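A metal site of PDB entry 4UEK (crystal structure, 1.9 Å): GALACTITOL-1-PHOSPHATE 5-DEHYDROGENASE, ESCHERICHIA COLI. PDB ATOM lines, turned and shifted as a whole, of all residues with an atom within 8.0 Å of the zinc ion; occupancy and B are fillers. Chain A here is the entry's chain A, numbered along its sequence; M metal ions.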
ATOM      1  N   LEU A  87       1.813 -23.659  27.962  1.00  0.00           N
ATOM      2  CA  LEU A  87       2.654 -23.440  26.785  1.00  0.00           C
ATOM      3  C   LEU A  87       1.931 -23.905  25.532  1.00  0.00           C
ATOM      4  O   LEU A  87       1.951 -25.081  25.214  1.00  0.00           O
ATOM      5  CB  LEU A  87       3.997 -24.175  26.911  1.00  0.00           C
ATOM      6  CG  LEU A  87       4.997 -23.955  25.778  1.00  0.00           C
ATOM      7  CD1 LEU A  87       5.499 -22.515  25.737  1.00  0.00           C
ATOM      8  CD2 LEU A  87       6.162 -24.930  25.891  1.00  0.00           C
ATOM      9  N   PRO A  88       1.269 -22.976  24.808  1.00  0.00           N
ATOM     10  CA  PRO A  88       0.614 -23.388  23.565  1.00  0.00           C
ATOM     11  C   PRO A  88       1.658 -23.577  22.449  1.00  0.00           C
ATOM     12  O   PRO A  88       2.829 -23.265  22.671  1.00  0.00           O
ATOM     13  CB  PRO A  88      -0.328 -22.215  23.266  1.00  0.00           C
ATOM     14  CG  PRO A  88       0.314 -21.046  23.906  1.00  0.00           C
ATOM     15  CD  PRO A  88       1.125 -21.541  25.080  1.00  0.00           C
ATOM     16  N   CYS A  89       1.250 -24.073  21.288  1.00  0.00           N
ATOM     17  CA  CYS A  89       2.214 -24.319  20.203  1.00  0.00           C
ATOM     18  C   CYS A  89       2.486 -23.073  19.345  1.00  0.00           C
ATOM     19  O   CYS A  89       3.499 -23.016  18.661  1.00  0.00           O
ATOM     20  CB  CYS A  89       1.739 -25.474  19.316  1.00  0.00           C
ATOM     21  SG  CYS A  89       0.502 -25.044  18.073  1.00  0.00           S
ATOM     22  N   PHE A  90       1.566 -22.120  19.374  1.00  0.00           N
ATOM     23  CA  PHE A  90       1.628 -20.856  18.612  1.00  0.00           C
ATOM     24  C   PHE A  90       1.599 -20.995  17.087  1.00  0.00           C
ATOM     25  O   PHE A  90       1.804 -20.003  16.378  1.00  0.00           O
ATOM     26  CB  PHE A  90       2.867 -20.043  19.035  1.00  0.00           C
ATOM     27  CG  PHE A  90       2.867 -19.638  20.483  1.00  0.00           C
ATOM     28  CD1 PHE A  90       1.934 -18.716  20.961  1.00  0.00           C
ATOM     29  CD2 PHE A  90       3.757 -20.208  21.386  1.00  0.00           C
ATOM     30  CE1 PHE A  90       1.904 -18.363  22.302  1.00  0.00           C
ATOM     31  CE2 PHE A  90       3.740 -19.855  22.734  1.00  0.00           C
ATOM     32  CZ  PHE A  90       2.824 -18.935  23.194  1.00  0.00           C
ATOM     33  N   THR A  91       1.320 -22.176  16.557  1.00  0.00           N
ATOM     34  CA  THR A  91       1.336 -22.364  15.097  1.00  0.00           C
ATOM     35  C   THR A  91       0.097 -23.051  14.507  1.00  0.00           C
ATOM     36  O   THR A  91      -0.030 -23.122  13.274  1.00  0.00           O
ATOM     37  CB  THR A  91       2.558 -23.183  14.666  1.00  0.00           C
ATOM     38  OG1 THR A  91       2.463 -24.494  15.229  1.00  0.00           O
ATOM     39  CG2 THR A  91       3.840 -22.520  15.131  1.00  0.00           C
ATOM     40  N   CYS A  92      -0.792 -23.547  15.366  1.00  0.00           N
ATOM     41  CA  CYS A  92      -2.087 -24.089  14.887  1.00  0.00           C
ATOM     42  C   CYS A  92      -3.118 -22.963  14.609  1.00  0.00           C
ATOM     43  O   CYS A  92      -2.912 -21.811  15.008  1.00  0.00           O
ATOM     44  CB  CYS A  92      -2.649 -25.087  15.899  1.00  0.00           C
ATOM     45  SG  CYS A  92      -3.203 -24.354  17.453  1.00  0.00           S
ATOM     46  N   PRO A  93      -4.223 -23.290  13.918  1.00  0.00           N
ATOM     47  CA  PRO A  93      -5.205 -22.227  13.629  1.00  0.00           C
ATOM     48  C   PRO A  93      -5.811 -21.603  14.887  1.00  0.00           C
ATOM     49  O   PRO A  93      -6.068 -20.402  14.900  1.00  0.00           O
ATOM     50  CB  PRO A  93      -6.265 -22.963  12.806  1.00  0.00           C
ATOM     51  CG  PRO A  93      -5.499 -24.076  12.134  1.00  0.00           C
ATOM     52  CD  PRO A  93      -4.509 -24.522  13.170  1.00  0.00           C
ATOM     53  N   GLU A  94      -6.013 -22.395  15.938  1.00  0.00           N
ATOM     54  CA  GLU A  94      -6.516 -21.891  17.216  1.00  0.00           C
ATOM     55  C   GLU A  94      -5.575 -20.832  17.809  1.00  0.00           C
ATOM     56  O   GLU A  94      -6.021 -19.748  18.205  1.00  0.00           O
ATOM     57  CB  GLU A  94      -6.708 -23.038  18.211  1.00  0.00           C
ATOM     58  CG  GLU A  94      -8.021 -23.831  18.041  1.00  0.00           C
ATOM     59  CD  GLU A  94      -7.987 -24.891  16.937  1.00  0.00           C
ATOM     60  OE1 GLU A  94      -7.008 -24.965  16.164  1.00  0.00           O
ATOM     61  OE2 GLU A  94      -8.962 -25.658  16.818  1.00  0.00           O
ATOM     62  N   CYS A  95      -4.277 -21.140  17.855  1.00  0.00           N
ATOM     63  CA  CYS A  95      -3.258 -20.207  18.389  1.00  0.00           C
ATOM     64  C   CYS A  95      -3.150 -18.935  17.548  1.00  0.00           C
ATOM     65  O   CYS A  95      -3.032 -17.824  18.079  1.00  0.00           O
ATOM     66  CB  CYS A  95      -1.896 -20.905  18.460  1.00  0.00           C
ATOM     67  SG  CYS A  95      -1.634 -22.021  19.887  1.00  0.00           S
ATOM     68  N   LEU A  96      -3.182 -19.094  16.225  1.00  0.00           N
ATOM     69  CA  LEU A  96      -3.147 -17.967  15.293  1.00  0.00           C
ATOM     70  C   LEU A  96      -4.377 -17.068  15.473  1.00  0.00           C
ATOM     71  O   LEU A  96      -4.366 -15.903  15.086  1.00  0.00           O
ATOM     72  CB  LEU A  96      -3.053 -18.468  13.836  1.00  0.00           C
ATOM     73  CG  LEU A  96      -1.769 -19.270  13.554  1.00  0.00           C
ATOM     74  CD1 LEU A  96      -1.634 -19.622  12.076  1.00  0.00           C
ATOM     75  CD2 LEU A  96      -0.535 -18.525  14.048  1.00  0.00           C
ATOM     76  N   PHE A  99      -6.632 -18.122  20.404  1.00  0.00           N
ATOM     77  CA  PHE A  99      -7.378 -19.080  21.198  1.00  0.00           C
ATOM     78  C   PHE A  99      -6.422 -20.047  21.910  1.00  0.00           C
ATOM     79  O   PHE A  99      -6.535 -21.266  21.767  1.00  0.00           O
ATOM     80  CB  PHE A  99      -8.339 -19.883  20.310  1.00  0.00           C
ATOM     81  CG  PHE A  99      -9.435 -19.065  19.662  1.00  0.00           C
ATOM     82  CD1 PHE A  99      -9.742 -17.797  20.095  1.00  0.00           C
ATOM     83  CD2 PHE A  99     -10.182 -19.601  18.614  1.00  0.00           C
ATOM     84  CE1 PHE A  99     -10.766 -17.063  19.502  1.00  0.00           C
ATOM     85  CE2 PHE A  99     -11.188 -18.875  18.016  1.00  0.00           C
ATOM     86  CZ  PHE A  99     -11.476 -17.595  18.460  1.00  0.00           C
ATOM     87  N   TYR A 100      -5.486 -19.510  22.694  1.00  0.00           N
ATOM     88  CA  TYR A 100      -4.390 -20.343  23.210  1.00  0.00           C
ATOM     89  C   TYR A 100      -4.862 -21.544  24.047  1.00  0.00           C
ATOM     90  O   TYR A 100      -4.251 -22.623  24.012  1.00  0.00           O
ATOM     91  CB  TYR A 100      -3.429 -19.484  24.022  1.00  0.00           C
ATOM     92  CG  TYR A 100      -2.882 -18.315  23.254  1.00  0.00           C
ATOM     93  CD1 TYR A 100      -2.000 -18.505  22.197  1.00  0.00           C
ATOM     94  CD2 TYR A 100      -3.267 -17.006  23.559  1.00  0.00           C
ATOM     95  CE1 TYR A 100      -1.506 -17.441  21.465  1.00  0.00           C
ATOM     96  CE2 TYR A 100      -2.767 -15.931  22.832  1.00  0.00           C
ATOM     97  CZ  TYR A 100      -1.890 -16.153  21.799  1.00  0.00           C
ATOM     98  OH  TYR A 100      -1.387 -15.093  21.065  1.00  0.00           O
ATOM     99  N   SER A 101      -5.954 -21.389  24.785  1.00  0.00           N
ATOM    100  CA  SER A 101      -6.383 -22.465  25.675  1.00  0.00           C
ATOM    101  C   SER A 101      -7.157 -23.547  24.926  1.00  0.00           C
ATOM    102  O   SER A 101      -7.525 -24.569  25.499  1.00  0.00           O
ATOM    103  CB  SER A 101      -7.206 -21.908  26.857  1.00  0.00           C
ATOM    104  OG  SER A 101      -8.391 -21.266  26.443  1.00  0.00           O
ATOM    105  N   GLN A 102      -7.370 -23.334  23.624  1.00  0.00           N
ATOM    106  CA  GLN A 102      -7.917 -24.394  22.781  1.00  0.00           C
ATOM    107  C   GLN A 102      -6.837 -25.017  21.877  1.00  0.00           C
ATOM    108  O   GLN A 102      -7.163 -25.812  20.975  1.00  0.00           O
ATOM    109  CB  GLN A 102      -9.073 -23.848  21.920  1.00  0.00           C
ATOM    110  CG  GLN A 102     -10.356 -23.539  22.711  1.00  0.00           C
ATOM    111  CD  GLN A 102     -10.260 -22.297  23.595  1.00  0.00           C
ATOM    112  OE1 GLN A 102      -9.706 -21.271  23.192  1.00  0.00           O
ATOM    113  NE2 GLN A 102     -10.805 -22.386  24.807  1.00  0.00           N
ATOM    114  N   CYS A 103      -5.569 -24.668  22.113  1.00  0.00           N
ATOM    115  CA  CYS A 103      -4.459 -25.200  21.301  1.00  0.00           C
ATOM    116  C   CYS A 103      -4.467 -26.715  21.338  1.00  0.00           C
ATOM    117  O   CYS A 103      -4.570 -27.332  22.412  1.00  0.00           O
ATOM    118  CB  CYS A 103      -3.076 -24.708  21.770  1.00  0.00           C
ATOM    119  SG  CYS A 103      -1.688 -25.650  21.012  1.00  0.00           S
ATOM    120  N   ALA A 104      -4.328 -27.307  20.155  1.00  0.00           N
ATOM    121  CA  ALA A 104      -4.315 -28.757  20.024  1.00  0.00           C
ATOM    122  C   ALA A 104      -3.113 -29.393  20.713  1.00  0.00           C
ATOM    123  O   ALA A 104      -3.176 -30.538  21.162  1.00  0.00           O
ATOM    124  CB  ALA A 104      -4.346 -29.133  18.546  1.00  0.00           C
ATOM    125  N   LYS A 105      -2.031 -28.639  20.836  1.00  0.00           N
ATOM    126  CA  LYS A 105      -0.733 -29.205  21.186  1.00  0.00           C
ATOM    127  C   LYS A 105      -0.105 -28.613  22.437  1.00  0.00           C
ATOM    128  O   LYS A 105       1.108 -28.491  22.488  1.00  0.00           O
ATOM    129  CB  LYS A 105       0.237 -29.005  20.016  1.00  0.00           C
ATOM    130  CG  LYS A 105       0.256 -30.054  18.926  1.00  0.00           C
ATOM    131  CD  LYS A 105       1.709 -30.431  18.609  1.00  0.00           C
ATOM    132  CE  LYS A 105       1.831 -31.259  17.343  1.00  0.00           C
ATOM    133  NZ  LYS A 105       2.179 -32.684  17.561  1.00  0.00           N
ATOM    134  N   TYR A 106      -0.882 -28.229  23.440  1.00  0.00           N
ATOM    135  CA  TYR A 106      -0.286 -27.394  24.486  1.00  0.00           C
ATOM    136  C   TYR A 106       0.319 -28.196  25.636  1.00  0.00           C
ATOM    137  O   TYR A 106      -0.077 -29.320  25.913  1.00  0.00           O
ATOM    138  CB  TYR A 106      -1.297 -26.365  25.007  1.00  0.00           C
ATOM    139  CG  TYR A 106      -2.479 -26.833  25.857  1.00  0.00           C
ATOM    140  CD1 TYR A 106      -2.307 -27.213  27.166  1.00  0.00           C
ATOM    141  CD2 TYR A 106      -3.774 -26.809  25.335  1.00  0.00           C
ATOM    142  CE1 TYR A 106      -3.364 -27.590  27.942  1.00  0.00           C
ATOM    143  CE2 TYR A 106      -4.854 -27.190  26.112  1.00  0.00           C
ATOM    144  CZ  TYR A 106      -4.643 -27.581  27.419  1.00  0.00           C
ATOM    145  OH  TYR A 106      -5.697 -27.946  28.224  1.00  0.00           O
HETATM  146 ZN    ZN M   1      -1.515 -24.218  19.085  1.00  0.00          ZN
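The side-chain sulfur of Cys 95 sits close to the backbone NH of Phe 90, at 3.2 Å.
N of Glu 94 sits close to SG of Cys 92 (3.7 Å).
The side-chain sulfur (SG) of Cys 89 lies close to the backbone NH (N) of Thr 91.
SG of Cys 103 sits close to N of Lys 105 (3.0 Å).
The side-chain sulfur (SG) of Cys 103 sits close to the backbone NH (N) of Tyr 106 (3.6 Å).
Residues that only touch the zinc ion: Phe 90.
SG of Cys 95 is bound to the zinc ion (2.3 Å).
The side-chain sulfur (SG) of Cys 92 binds the zinc ion.
The zinc ion is bound by SG of Cys 89 (2.4 Å).
The zinc ion is bound by SG of Cys 103 (2.4 Å).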
